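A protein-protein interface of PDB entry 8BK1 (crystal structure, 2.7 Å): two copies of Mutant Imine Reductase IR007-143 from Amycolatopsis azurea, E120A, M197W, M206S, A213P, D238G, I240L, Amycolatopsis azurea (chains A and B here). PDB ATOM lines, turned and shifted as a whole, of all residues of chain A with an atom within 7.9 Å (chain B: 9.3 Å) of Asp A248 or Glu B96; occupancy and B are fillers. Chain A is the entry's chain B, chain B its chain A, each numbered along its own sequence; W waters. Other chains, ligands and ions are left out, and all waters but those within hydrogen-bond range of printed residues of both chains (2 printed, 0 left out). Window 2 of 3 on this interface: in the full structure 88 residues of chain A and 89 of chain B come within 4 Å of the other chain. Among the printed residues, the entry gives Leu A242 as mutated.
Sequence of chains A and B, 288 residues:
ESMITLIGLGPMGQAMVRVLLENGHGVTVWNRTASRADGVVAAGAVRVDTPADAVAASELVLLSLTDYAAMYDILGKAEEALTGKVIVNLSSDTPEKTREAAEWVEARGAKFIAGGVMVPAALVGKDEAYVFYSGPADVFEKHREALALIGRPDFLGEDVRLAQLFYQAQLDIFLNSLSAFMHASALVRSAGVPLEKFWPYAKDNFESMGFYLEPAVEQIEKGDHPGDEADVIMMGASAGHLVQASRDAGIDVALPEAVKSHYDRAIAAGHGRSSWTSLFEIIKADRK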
ATOM      1  N   LEU A 187      21.299 -22.238 -25.868  1.00  0.00           N
ATOM      2  CA  LEU A 187      21.273 -21.558 -24.553  1.00  0.00           C
ATOM      3  C   LEU A 187      19.925 -21.859 -23.891  1.00  0.00           C
ATOM      4  O   LEU A 187      19.855 -22.185 -22.675  1.00  0.00           O
ATOM      5  CB  LEU A 187      21.458 -20.053 -24.759  1.00  0.00           C
ATOM      6  CG  LEU A 187      21.488 -19.224 -23.480  1.00  0.00           C
ATOM      7  CD1 LEU A 187      22.767 -19.469 -22.711  1.00  0.00           C
ATOM      8  CD2 LEU A 187      21.400 -17.759 -23.816  1.00  0.00           C
ATOM      9  N   SER A 190      19.496 -25.561 -23.037  1.00  0.00           N
ATOM     10  CA  SER A 190      20.308 -25.825 -21.836  1.00  0.00           C
ATOM     11  C   SER A 190      19.482 -25.560 -20.574  1.00  0.00           C
ATOM     12  O   SER A 190      19.744 -26.179 -19.588  1.00  0.00           O
ATOM     13  CB  SER A 190      21.554 -25.007 -21.864  1.00  0.00           C
ATOM     14  OG  SER A 190      22.252 -25.128 -20.635  1.00  0.00           O
ATOM     15  N   HIS A 241      27.897 -10.530 -20.843  1.00  0.00           N
ATOM     16  CA  HIS A 241      26.766 -11.265 -20.236  1.00  0.00           C
ATOM     17  C   HIS A 241      26.540 -12.554 -21.047  1.00  0.00           C
ATOM     18  O   HIS A 241      26.519 -13.641 -20.433  1.00  0.00           O
ATOM     19  CB  HIS A 241      25.523 -10.361 -20.180  1.00  0.00           C
ATOM     20  CG  HIS A 241      25.751  -9.129 -19.382  1.00  0.00           C
ATOM     21  ND1 HIS A 241      25.026  -7.961 -19.581  1.00  0.00           N
ATOM     22  CD2 HIS A 241      26.637  -8.884 -18.389  1.00  0.00           C
ATOM     23  CE1 HIS A 241      25.463  -7.042 -18.732  1.00  0.00           C
ATOM     24  NE2 HIS A 241      26.460  -7.591 -17.984  1.00  0.00           N
ATOM     25  N   LEU A 242      26.479 -12.449 -22.378  1.00  0.00           N
ATOM     26  CA  LEU A 242      26.237 -13.626 -23.238  1.00  0.00           C
ATOM     27  C   LEU A 242      27.369 -14.631 -23.031  1.00  0.00           C
ATOM     28  O   LEU A 242      27.090 -15.827 -22.863  1.00  0.00           O
ATOM     29  CB  LEU A 242      26.134 -13.188 -24.697  1.00  0.00           C
ATOM     30  CG  LEU A 242      25.845 -14.325 -25.663  1.00  0.00           C
ATOM     31  CD1 LEU A 242      24.613 -15.069 -25.214  1.00  0.00           C
ATOM     32  CD2 LEU A 242      25.663 -13.789 -27.084  1.00  0.00           C
ATOM     33  N   VAL A 243      28.604 -14.151 -22.965  1.00  0.00           N
ATOM     34  CA  VAL A 243      29.771 -15.056 -22.810  1.00  0.00           C
ATOM     35  C   VAL A 243      29.624 -15.780 -21.462  1.00  0.00           C
ATOM     36  O   VAL A 243      29.714 -17.027 -21.468  1.00  0.00           O
ATOM     37  CB  VAL A 243      31.115 -14.306 -22.920  1.00  0.00           C
ATOM     38  CG1 VAL A 243      32.262 -15.157 -22.421  1.00  0.00           C
ATOM     39  CG2 VAL A 243      31.396 -13.818 -24.335  1.00  0.00           C
ATOM     40  N   GLN A 244      29.378 -15.046 -20.368  1.00  0.00           N
ATOM     41  CA  GLN A 244      29.283 -15.651 -19.019  1.00  0.00           C
ATOM     42  C   GLN A 244      28.094 -16.633 -19.013  1.00  0.00           C
ATOM     43  O   GLN A 244      28.249 -17.768 -18.527  1.00  0.00           O
ATOM     44  CB  GLN A 244      29.206 -14.557 -17.944  1.00  0.00           C
ATOM     45  CG  GLN A 244      29.358 -15.048 -16.498  1.00  0.00           C
ATOM     46  CD  GLN A 244      30.571 -15.934 -16.303  1.00  0.00           C
ATOM     47  OE1 GLN A 244      31.694 -15.481 -16.454  1.00  0.00           O
ATOM     48  NE2 GLN A 244      30.384 -17.219 -16.015  1.00  0.00           N
ATOM     49  N   ALA A 245      26.958 -16.251 -19.592  1.00  0.00           N
ATOM     50  CA  ALA A 245      25.734 -17.086 -19.599  1.00  0.00           C
ATOM     51  C   ALA A 245      26.030 -18.400 -20.315  1.00  0.00           C
ATOM     52  O   ALA A 245      25.489 -19.443 -19.891  1.00  0.00           O
ATOM     53  CB  ALA A 245      24.590 -16.345 -20.255  1.00  0.00           C
ATOM     54  N   SER A 246      26.828 -18.330 -21.382  1.00  0.00           N
ATOM     55  CA  SER A 246      27.222 -19.484 -22.219  1.00  0.00           C
ATOM     56  C   SER A 246      28.107 -20.419 -21.381  1.00  0.00           C
ATOM     57  O   SER A 246      27.865 -21.655 -21.427  1.00  0.00           O
ATOM     58  CB  SER A 246      27.897 -19.011 -23.481  1.00  0.00           C
ATOM     59  OG  SER A 246      26.978 -18.331 -24.318  1.00  0.00           O
ATOM     60  N   ARG A 247      29.089 -19.876 -20.647  1.00  0.00           N
ATOM     61  CA  ARG A 247      29.939 -20.704 -19.743  1.00  0.00           C
ATOM     62  C   ARG A 247      29.026 -21.376 -18.708  1.00  0.00           C
ATOM     63  O   ARG A 247      29.076 -22.589 -18.593  1.00  0.00           O
ATOM     64  CB  ARG A 247      31.006 -19.922 -18.985  1.00  0.00           C
ATOM     65  CG  ARG A 247      32.094 -19.287 -19.828  1.00  0.00           C
ATOM     66  CD  ARG A 247      33.401 -19.152 -19.075  1.00  0.00           C
ATOM     67  NE  ARG A 247      34.265 -18.357 -19.949  1.00  0.00           N
ATOM     68  CZ  ARG A 247      34.368 -17.029 -19.920  1.00  0.00           C
ATOM     69  NH1 ARG A 247      33.681 -16.309 -19.042  1.00  0.00           N
ATOM     70  NH2 ARG A 247      35.167 -16.417 -20.788  1.00  0.00           N
ATOM     71  N   ASP A 248      28.200 -20.596 -18.006  1.00  0.00           N
ATOM     72  CA  ASP A 248      27.196 -21.065 -17.008  1.00  0.00           C
ATOM     73  C   ASP A 248      26.387 -22.238 -17.590  1.00  0.00           C
ATOM     74  O   ASP A 248      26.216 -23.200 -16.889  1.00  0.00           O
ATOM     75  CB  ASP A 248      26.276 -19.922 -16.580  1.00  0.00           C
ATOM     76  CG  ASP A 248      26.976 -18.910 -15.700  1.00  0.00           C
ATOM     77  OD1 ASP A 248      28.184 -19.156 -15.387  1.00  0.00           O
ATOM     78  OD2 ASP A 248      26.324 -17.882 -15.347  1.00  0.00           O
ATOM     79  N   ALA A 249      25.961 -22.179 -18.848  1.00  0.00           N
ATOM     80  CA  ALA A 249      25.069 -23.178 -19.483  1.00  0.00           C
ATOM     81  C   ALA A 249      25.869 -24.378 -20.034  1.00  0.00           C
ATOM     82  O   ALA A 249      25.223 -25.332 -20.509  1.00  0.00           O
ATOM     83  CB  ALA A 249      24.250 -22.495 -20.566  1.00  0.00           C
ATOM     84  N   GLY A 250      27.205 -24.306 -20.047  1.00  0.00           N
ATOM     85  CA  GLY A 250      28.073 -25.287 -20.728  1.00  0.00           C
ATOM     86  C   GLY A 250      27.897 -25.380 -22.242  1.00  0.00           C
ATOM     87  O   GLY A 250      28.237 -26.407 -22.798  1.00  0.00           O
ATOM     88  N   ILE A 251      27.508 -24.315 -22.934  1.00  0.00           N
ATOM     89  CA  ILE A 251      27.449 -24.327 -24.435  1.00  0.00           C
ATOM     90  C   ILE A 251      28.716 -23.719 -25.032  1.00  0.00           C
ATOM     91  O   ILE A 251      29.576 -23.230 -24.254  1.00  0.00           O
ATOM     92  CB  ILE A 251      26.195 -23.598 -24.917  1.00  0.00           C
ATOM     93  CG1 ILE A 251      26.257 -22.083 -24.662  1.00  0.00           C
ATOM     94  CG2 ILE A 251      24.975 -24.248 -24.262  1.00  0.00           C
ATOM     95  CD1 ILE A 251      25.090 -21.331 -25.273  1.00  0.00           C
ATOM     96  N   VAL A 253      31.475 -21.329 -26.397  1.00  0.00           N
ATOM     97  CA  VAL A 253      31.899 -19.944 -26.062  1.00  0.00           C
ATOM     98  C   VAL A 253      32.686 -19.296 -27.217  1.00  0.00           C
ATOM     99  O   VAL A 253      32.923 -18.059 -27.136  1.00  0.00           O
ATOM    100  CB  VAL A 253      32.709 -19.896 -24.749  1.00  0.00           C
ATOM    101  CG1 VAL A 253      31.849 -20.305 -23.585  1.00  0.00           C
ATOM    102  CG2 VAL A 253      33.978 -20.727 -24.793  1.00  0.00           C
ATOM    103  N   TYR B  68      23.838  -5.591 -13.634  1.00  0.00           N
ATOM    104  CA  TYR B  68      23.280  -5.844 -12.281  1.00  0.00           C
ATOM    105  C   TYR B  68      24.260  -5.301 -11.229  1.00  0.00           C
ATOM    106  O   TYR B  68      23.790  -4.774 -10.212  1.00  0.00           O
ATOM    107  CB  TYR B  68      22.875  -7.311 -12.116  1.00  0.00           C
ATOM    108  CG  TYR B  68      21.463  -7.623 -12.577  1.00  0.00           C
ATOM    109  CD1 TYR B  68      20.934  -7.080 -13.742  1.00  0.00           C
ATOM    110  CD2 TYR B  68      20.650  -8.489 -11.861  1.00  0.00           C
ATOM    111  CE1 TYR B  68      19.637  -7.353 -14.154  1.00  0.00           C
ATOM    112  CE2 TYR B  68      19.361  -8.785 -12.267  1.00  0.00           C
ATOM    113  CZ  TYR B  68      18.841  -8.219 -13.424  1.00  0.00           C
ATOM    114  OH  TYR B  68      17.557  -8.502 -13.831  1.00  0.00           O
ATOM    115  N   TYR B  72      23.476  -3.194  -7.388  1.00  0.00           N
ATOM    116  CA  TYR B  72      24.078  -3.353  -6.047  1.00  0.00           C
ATOM    117  C   TYR B  72      24.700  -2.014  -5.622  1.00  0.00           C
ATOM    118  O   TYR B  72      24.478  -1.594  -4.490  1.00  0.00           O
ATOM    119  CB  TYR B  72      25.051  -4.517  -6.037  1.00  0.00           C
ATOM    120  CG  TYR B  72      24.448  -5.888  -6.238  1.00  0.00           C
ATOM    121  CD1 TYR B  72      23.555  -6.414  -5.329  1.00  0.00           C
ATOM    122  CD2 TYR B  72      24.817  -6.694  -7.305  1.00  0.00           C
ATOM    123  CE1 TYR B  72      23.018  -7.690  -5.489  1.00  0.00           C
ATOM    124  CE2 TYR B  72      24.307  -7.968  -7.469  1.00  0.00           C
ATOM    125  CZ  TYR B  72      23.386  -8.473  -6.565  1.00  0.00           C
ATOM    126  OH  TYR B  72      22.867  -9.728  -6.758  1.00  0.00           O
ATOM    127  N   ASP B  93      22.041  -8.874 -17.944  1.00  0.00           N
ATOM    128  CA  ASP B  93      23.102  -9.589 -17.182  1.00  0.00           C
ATOM    129  C   ASP B  93      22.881 -11.095 -17.382  1.00  0.00           C
ATOM    130  O   ASP B  93      22.049 -11.464 -18.222  1.00  0.00           O
ATOM    131  CB  ASP B  93      23.166  -9.150 -15.714  1.00  0.00           C
ATOM    132  CG  ASP B  93      24.570  -9.136 -15.115  1.00  0.00           C
ATOM    133  OD1 ASP B  93      25.270 -10.187 -15.184  1.00  0.00           O
ATOM    134  OD2 ASP B  93      24.974  -8.067 -14.615  1.00  0.00           O
ATOM    135  N   THR B  94      23.583 -11.952 -16.647  1.00  0.00           N
ATOM    136  CA  THR B  94      23.414 -13.421 -16.810  1.00  0.00           C
ATOM    137  C   THR B  94      22.142 -13.846 -16.091  1.00  0.00           C
ATOM    138  O   THR B  94      21.777 -13.218 -15.098  1.00  0.00           O
ATOM    139  CB  THR B  94      24.624 -14.185 -16.279  1.00  0.00           C
ATOM    140  OG1 THR B  94      24.555 -14.103 -14.856  1.00  0.00           O
ATOM    141  CG2 THR B  94      25.924 -13.613 -16.790  1.00  0.00           C
ATOM    142  N   PRO B  95      21.453 -14.919 -16.548  1.00  0.00           N
ATOM    143  CA  PRO B  95      20.400 -15.551 -15.758  1.00  0.00           C
ATOM    144  C   PRO B  95      20.820 -15.886 -14.318  1.00  0.00           C
ATOM    145  O   PRO B  95      20.079 -15.538 -13.424  1.00  0.00           O
ATOM    146  CB  PRO B  95      20.098 -16.822 -16.555  1.00  0.00           C
ATOM    147  CG  PRO B  95      20.374 -16.404 -17.965  1.00  0.00           C
ATOM    148  CD  PRO B  95      21.611 -15.548 -17.859  1.00  0.00           C
ATOM    149  N   GLU B  96      21.983 -16.508 -14.116  1.00  0.00           N
ATOM    150  CA  GLU B  96      22.459 -16.852 -12.748  1.00  0.00           C
ATOM    151  C   GLU B  96      22.522 -15.581 -11.886  1.00  0.00           C
ATOM    152  O   GLU B  96      22.068 -15.633 -10.726  1.00  0.00           O
ATOM    153  CB  GLU B  96      23.762 -17.664 -12.781  1.00  0.00           C
ATOM    154  CG  GLU B  96      23.518 -19.174 -12.980  1.00  0.00           C
ATOM    155  CD  GLU B  96      22.275 -19.730 -12.257  1.00  0.00           C
ATOM    156  OE1 GLU B  96      22.283 -19.733 -10.996  1.00  0.00           O
ATOM    157  OE2 GLU B  96      21.252 -20.084 -12.935  1.00  0.00           O
ATOM    158  N   LYS B  97      23.011 -14.456 -12.405  1.00  0.00           N
ATOM    159  CA  LYS B  97      23.155 -13.241 -11.563  1.00  0.00           C
ATOM    160  C   LYS B  97      21.772 -12.624 -11.379  1.00  0.00           C
ATOM    161  O   LYS B  97      21.581 -11.932 -10.380  1.00  0.00           O
ATOM    162  CB  LYS B  97      24.180 -12.254 -12.131  1.00  0.00           C
ATOM    163  CG  LYS B  97      25.623 -12.636 -11.858  1.00  0.00           C
ATOM    164  CD  LYS B  97      26.651 -11.574 -12.180  1.00  0.00           C
ATOM    165  CE  LYS B  97      27.779 -11.547 -11.165  1.00  0.00           C
ATOM    166  NZ  LYS B  97      28.985 -10.985 -11.789  1.00  0.00           N
ATOM    167  N   THR B  98      20.839 -12.885 -12.291  1.00  0.00           N
ATOM    168  CA  THR B  98      19.439 -12.400 -12.171  1.00  0.00           C
ATOM    169  C   THR B  98      18.797 -13.076 -10.954  1.00  0.00           C
ATOM    170  O   THR B  98      18.156 -12.401 -10.170  1.00  0.00           O
ATOM    171  CB  THR B  98      18.642 -12.571 -13.469  1.00  0.00           C
ATOM    172  OG1 THR B  98      19.239 -11.832 -14.547  1.00  0.00           O
ATOM    173  CG2 THR B  98      17.215 -12.080 -13.287  1.00  0.00           C
ATOM    174  N   ARG B  99      18.978 -14.378 -10.777  1.00  0.00           N
ATOM    175  CA  ARG B  99      18.393 -15.080  -9.619  1.00  0.00           C
ATOM    176  C   ARG B  99      19.088 -14.628  -8.334  1.00  0.00           C
ATOM    177  O   ARG B  99      18.381 -14.410  -7.338  1.00  0.00           O
ATOM    178  CB  ARG B  99      18.551 -16.585  -9.736  1.00  0.00           C
ATOM    179  CG  ARG B  99      18.155 -17.297  -8.464  1.00  0.00           C
ATOM    180  CD  ARG B  99      17.746 -18.693  -8.784  1.00  0.00           C
ATOM    181  NE  ARG B  99      18.936 -19.425  -9.086  1.00  0.00           N
ATOM    182  CZ  ARG B  99      18.952 -20.729  -9.345  1.00  0.00           C
ATOM    183  NH1 ARG B  99      17.813 -21.407  -9.355  1.00  0.00           N
ATOM    184  NH2 ARG B  99      20.103 -21.343  -9.601  1.00  0.00           N
ATOM    185  N   GLU B 100      20.414 -14.482  -8.356  1.00  0.00           N
ATOM    186  CA  GLU B 100      21.170 -14.071  -7.155  1.00  0.00           C
ATOM    187  C   GLU B 100      20.634 -12.697  -6.712  1.00  0.00           C
ATOM    188  O   GLU B 100      20.482 -12.468  -5.496  1.00  0.00           O
ATOM    189  CB  GLU B 100      22.670 -14.208  -7.405  1.00  0.00           C
ATOM    190  CG  GLU B 100      23.499 -13.250  -6.575  1.00  0.00           C
ATOM    191  CD  GLU B 100      24.964 -13.175  -6.996  1.00  0.00           C
ATOM    192  OE1 GLU B 100      25.318 -12.402  -7.920  1.00  0.00           O
ATOM    193  OE2 GLU B 100      25.736 -13.904  -6.413  1.00  0.00           O
ATOM    194  N   ALA B 101      20.258 -11.825  -7.644  1.00  0.00           N
ATOM    195  CA  ALA B 101      19.858 -10.442  -7.313  1.00  0.00           C
ATOM    196  C   ALA B 101      18.435 -10.470  -6.769  1.00  0.00           C
ATOM    197  O   ALA B 101      18.129  -9.677  -5.851  1.00  0.00           O
ATOM    198  CB  ALA B 101      19.985  -9.534  -8.505  1.00  0.00           C
ATOM    199  N   ALA B 102      17.593 -11.360  -7.296  1.00  0.00           N
ATOM    200  CA  ALA B 102      16.215 -11.533  -6.798  1.00  0.00           C
ATOM    201  C   ALA B 102      16.283 -11.927  -5.314  1.00  0.00           C
ATOM    202  O   ALA B 102      15.566 -11.344  -4.509  1.00  0.00           O
ATOM    203  CB  ALA B 102      15.494 -12.548  -7.636  1.00  0.00           C
ATOM    204  N   GLU B 103      17.164 -12.850  -4.960  1.00  0.00           N
ATOM    205  CA  GLU B 103      17.316 -13.340  -3.566  1.00  0.00           C
ATOM    206  C   GLU B 103      17.785 -12.184  -2.671  1.00  0.00           C
ATOM    207  O   GLU B 103      17.258 -12.031  -1.566  1.00  0.00           O
ATOM    208  CB  GLU B 103      18.245 -14.553  -3.535  1.00  0.00           C
ATOM    209  CG  GLU B 103      17.542 -15.809  -4.026  1.00  0.00           C
ATOM    210  CD  GLU B 103      18.435 -16.990  -4.378  1.00  0.00           C
ATOM    211  OE1 GLU B 103      19.644 -16.940  -4.079  1.00  0.00           O
ATOM    212  OE2 GLU B 103      17.921 -17.945  -4.980  1.00  0.00           O
ATOM    213  N   PHE B 112      10.897  -8.805  -6.532  1.00  0.00           N
ATOM    214  CA  PHE B 112      11.793  -8.655  -7.698  1.00  0.00           C
ATOM    215  C   PHE B 112      11.172  -9.295  -8.935  1.00  0.00           C
ATOM    216  O   PHE B 112      10.854 -10.493  -8.947  1.00  0.00           O
ATOM    217  CB  PHE B 112      13.139  -9.305  -7.409  1.00  0.00           C
ATOM    218  CG  PHE B 112      14.179  -8.954  -8.431  1.00  0.00           C
ATOM    219  CD1 PHE B 112      14.292  -9.687  -9.599  1.00  0.00           C
ATOM    220  CD2 PHE B 112      15.028  -7.872  -8.222  1.00  0.00           C
ATOM    221  CE1 PHE B 112      15.265  -9.360 -10.532  1.00  0.00           C
ATOM    222  CE2 PHE B 112      15.991  -7.548  -9.156  1.00  0.00           C
ATOM    223  CZ  PHE B 112      16.104  -8.290 -10.313  1.00  0.00           C
ATOM    224  N   ASP B 159       9.779 -18.346 -12.683  1.00  0.00           N
ATOM    225  CA  ASP B 159      11.254 -18.451 -12.583  1.00  0.00           C
ATOM    226  C   ASP B 159      11.848 -17.122 -13.067  1.00  0.00           C
ATOM    227  O   ASP B 159      11.761 -16.791 -14.301  1.00  0.00           O
ATOM    228  CB  ASP B 159      11.831 -19.622 -13.378  1.00  0.00           C
ATOM    229  CG  ASP B 159      13.306 -19.890 -13.106  1.00  0.00           C
ATOM    230  OD1 ASP B 159      13.964 -19.069 -12.469  1.00  0.00           O
ATOM    231  OD2 ASP B 159      13.762 -20.971 -13.464  1.00  0.00           O
ATOM    232  N   VAL B 160      12.393 -16.356 -12.127  1.00  0.00           N
ATOM    233  CA  VAL B 160      12.803 -14.951 -12.386  1.00  0.00           C
ATOM    234  C   VAL B 160      13.870 -14.918 -13.500  1.00  0.00           C
ATOM    235  O   VAL B 160      13.964 -13.934 -14.215  1.00  0.00           O
ATOM    236  CB  VAL B 160      13.272 -14.321 -11.070  1.00  0.00           C
ATOM    237  CG1 VAL B 160      14.639 -14.832 -10.649  1.00  0.00           C
ATOM    238  CG2 VAL B 160      13.220 -12.820 -11.167  1.00  0.00           C
ATOM    239  N   ARG B 161      14.590 -16.007 -13.714  1.00  0.00           N
ATOM    240  CA  ARG B 161      15.618 -16.106 -14.784  1.00  0.00           C
ATOM    241  C   ARG B 161      15.043 -16.045 -16.207  1.00  0.00           C
ATOM    242  O   ARG B 161      15.824 -15.777 -17.132  1.00  0.00           O
ATOM    243  CB  ARG B 161      16.405 -17.399 -14.584  1.00  0.00           C
ATOM    244  CG  ARG B 161      17.181 -17.367 -13.277  1.00  0.00           C
ATOM    245  CD  ARG B 161      17.877 -18.672 -12.998  1.00  0.00           C
ATOM    246  NE  ARG B 161      16.902 -19.731 -12.990  1.00  0.00           N
ATOM    247  CZ  ARG B 161      17.175 -21.002 -12.754  1.00  0.00           C
ATOM    248  NH1 ARG B 161      18.407 -21.400 -12.521  1.00  0.00           N
ATOM    249  NH2 ARG B 161      16.204 -21.886 -12.723  1.00  0.00           N
ATOM    250  N   LEU B 162      13.763 -16.317 -16.429  1.00  0.00           N
ATOM    251  CA  LEU B 162      13.289 -16.594 -17.812  1.00  0.00           C
ATOM    252  C   LEU B 162      13.418 -15.346 -18.681  1.00  0.00           C
ATOM    253  O   LEU B 162      13.838 -15.479 -19.827  1.00  0.00           O
ATOM    254  CB  LEU B 162      11.851 -17.112 -17.792  1.00  0.00           C
ATOM    255  CG  LEU B 162      11.690 -18.580 -17.373  1.00  0.00           C
ATOM    256  CD1 LEU B 162      10.237 -18.863 -17.044  1.00  0.00           C
ATOM    257  CD2 LEU B 162      12.181 -19.514 -18.467  1.00  0.00           C
ATOM    258  N   GLN B 164      15.547 -12.935 -18.546  1.00  0.00           N
ATOM    259  CA  GLN B 164      16.982 -12.714 -18.834  1.00  0.00           C
ATOM    260  C   GLN B 164      17.450 -13.727 -19.880  1.00  0.00           C
ATOM    261  O   GLN B 164      18.133 -13.344 -20.847  1.00  0.00           O
ATOM    262  CB  GLN B 164      17.816 -12.780 -17.563  1.00  0.00           C
ATOM    263  CG  GLN B 164      19.185 -12.164 -17.759  1.00  0.00           C
ATOM    264  CD  GLN B 164      19.138 -10.664 -17.899  1.00  0.00           C
ATOM    265  OE1 GLN B 164      19.147  -9.924 -16.908  1.00  0.00           O
ATOM    266  NE2 GLN B 164      19.095 -10.211 -19.146  1.00  0.00           N
ATOM    267  N   LEU B 165      17.031 -14.971 -19.725  1.00  0.00           N
ATOM    268  CA  LEU B 165      17.390 -16.041 -20.681  1.00  0.00           C
ATOM    269  C   LEU B 165      16.926 -15.657 -22.083  1.00  0.00           C
ATOM    270  O   LEU B 165      17.734 -15.750 -23.038  1.00  0.00           O
ATOM    271  CB  LEU B 165      16.717 -17.338 -20.238  1.00  0.00           C
ATOM    272  CG  LEU B 165      16.952 -18.500 -21.182  1.00  0.00           C
ATOM    273  CD1 LEU B 165      18.369 -19.026 -21.090  1.00  0.00           C
ATOM    274  CD2 LEU B 165      15.966 -19.581 -20.862  1.00  0.00           C
ATOM    275  N   GLN B 168      18.921 -12.669 -23.450  1.00  0.00           N
ATOM    276  CA  GLN B 168      20.285 -13.072 -23.876  1.00  0.00           C
ATOM    277  C   GLN B 168      20.206 -13.865 -25.185  1.00  0.00           C
ATOM    278  O   GLN B 168      21.107 -13.728 -26.026  1.00  0.00           O
ATOM    279  CB  GLN B 168      20.966 -13.885 -22.767  1.00  0.00           C
ATOM    280  CG  GLN B 168      21.301 -13.087 -21.512  1.00  0.00           C
ATOM    281  CD  GLN B 168      22.089 -11.826 -21.771  1.00  0.00           C
ATOM    282  OE1 GLN B 168      23.111 -11.826 -22.461  1.00  0.00           O
ATOM    283  NE2 GLN B 168      21.616 -10.726 -21.210  1.00  0.00           N
ATOM    284  N   ALA B 285      25.036 -28.093 -24.684  1.00  0.00           N
ATOM    285  CA  ALA B 285      25.624 -28.653 -23.433  1.00  0.00           C
ATOM    286  C   ALA B 285      25.538 -30.178 -23.493  1.00  0.00           C
ATOM    287  O   ALA B 285      24.537 -30.691 -24.072  1.00  0.00           O
ATOM    288  CB  ALA B 285      24.868 -28.116 -22.240  1.00  0.00           C
HETATM  289  O   HOH W   1      23.741 -17.630 -16.385  1.00  0.00           O
HETATM  290  O   HOH W   2      26.589 -15.620 -14.093  1.00  0.00           O
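Printed residues of chain B within 4 Å of Asp A248: Glu B96.
Ala A249 touches just one residue of chain B: Ala B285 (3.3 Å).
Of the printed residues of chain A, Asp B93 touches His A241 (3.5 Å).
Printed residues of chain A within 4 Å of Thr B94: His A241 (3.7 Å), Gln A244 (3.6 Å) and Ala A245 (3.98 Å).
Of the printed residues of chain B, Ile A251 touches Ala B285.
Tyr B68 touches none of the printed residues of chain A.
The nearest residue of chain A that does not touch Glu B96 is Ala A245 (6.7 Å).
Water W2 bridges the side-chain carboxylate (OD2) of Asp A248 and the side-chain hydroxyl (OG1) of Thr B94.
Water W1 lies within hydrogen-bond range of the side-chain carboxylate of Asp A248 (2.8 Å) and the backbone NH of Glu B96 (3.1 Å).
No position is printed for both chains.
The side-chain hydroxyl of Ser A190 is in hydrogen-bond range of the backbone carbonyl oxygen of Ala A249 (3.0 Å).
N of Asp B93 lies within hydrogen-bond range of OE1 of Gln B164 (3.2 Å).
The side-chain amide nitrogen (NE2) of Gln B168 sits close to the side-chain amide nitrogen (NE2) of Gln B164, at 3.3 Å.
The guanidinium group (NH1) of Arg B161 is in salt-bridge range of the side-chain carboxylate (OE2) of Glu B96 (3.2 Å).
O of Asp B93 sits at hydrogen-bond distance from NE2 of Gln B168.
The backbone NH (N) of Ile A251 lies within hydrogen-bond range of the backbone carbonyl oxygen (O) of Ser A246, 3.1 Å away.
OE1 of Gln B168 lies within hydrogen-bond range of N of Leu A242 (3.4 Å).
Leu A187 touches Leu B165 (O to CD1, 3.8 Å).
CA of Asp B93 touches CG of His A241, 3.5 Å away.
Thr B94 touches His A241 (CG2 to O, 3.7 Å).
His A241 touches Gln B168 (CB to OE1, 3.6 Å).
Gln A244 touches Thr B94 (CB to CG2, 3.6 Å).
Ala A245 touches Thr B94 (N to CG2, 3.98 Å).
Ala A245 touches Pro B95.
Ala B285 touches Ala A249.
Gly A250 touches Ala B285 (O to CA, 3.5 Å).
Ile A251 touches Ala B285.
Printed residues of chain B that touch a printed residue of chain A: Asp B93, Thr B94, Pro B95, Glu B96, Leu B165, Gln B168 and Ala B285.
Of the 14 printed residues of chain A, 9 touch a printed residue of chain B.
Printed residues of chain A that touch a printed residue of chain B: Leu A187, His A241, Leu A242, Gln A244, Ala A245, Asp A248, Ala A249, Gly A250 and Ile A251.
Hydrophobic or aromatic side chains of chain A within 4 Å of the printed part of chain B: Leu A187, His A241, Leu A242, Ala A245 and Ile A251.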
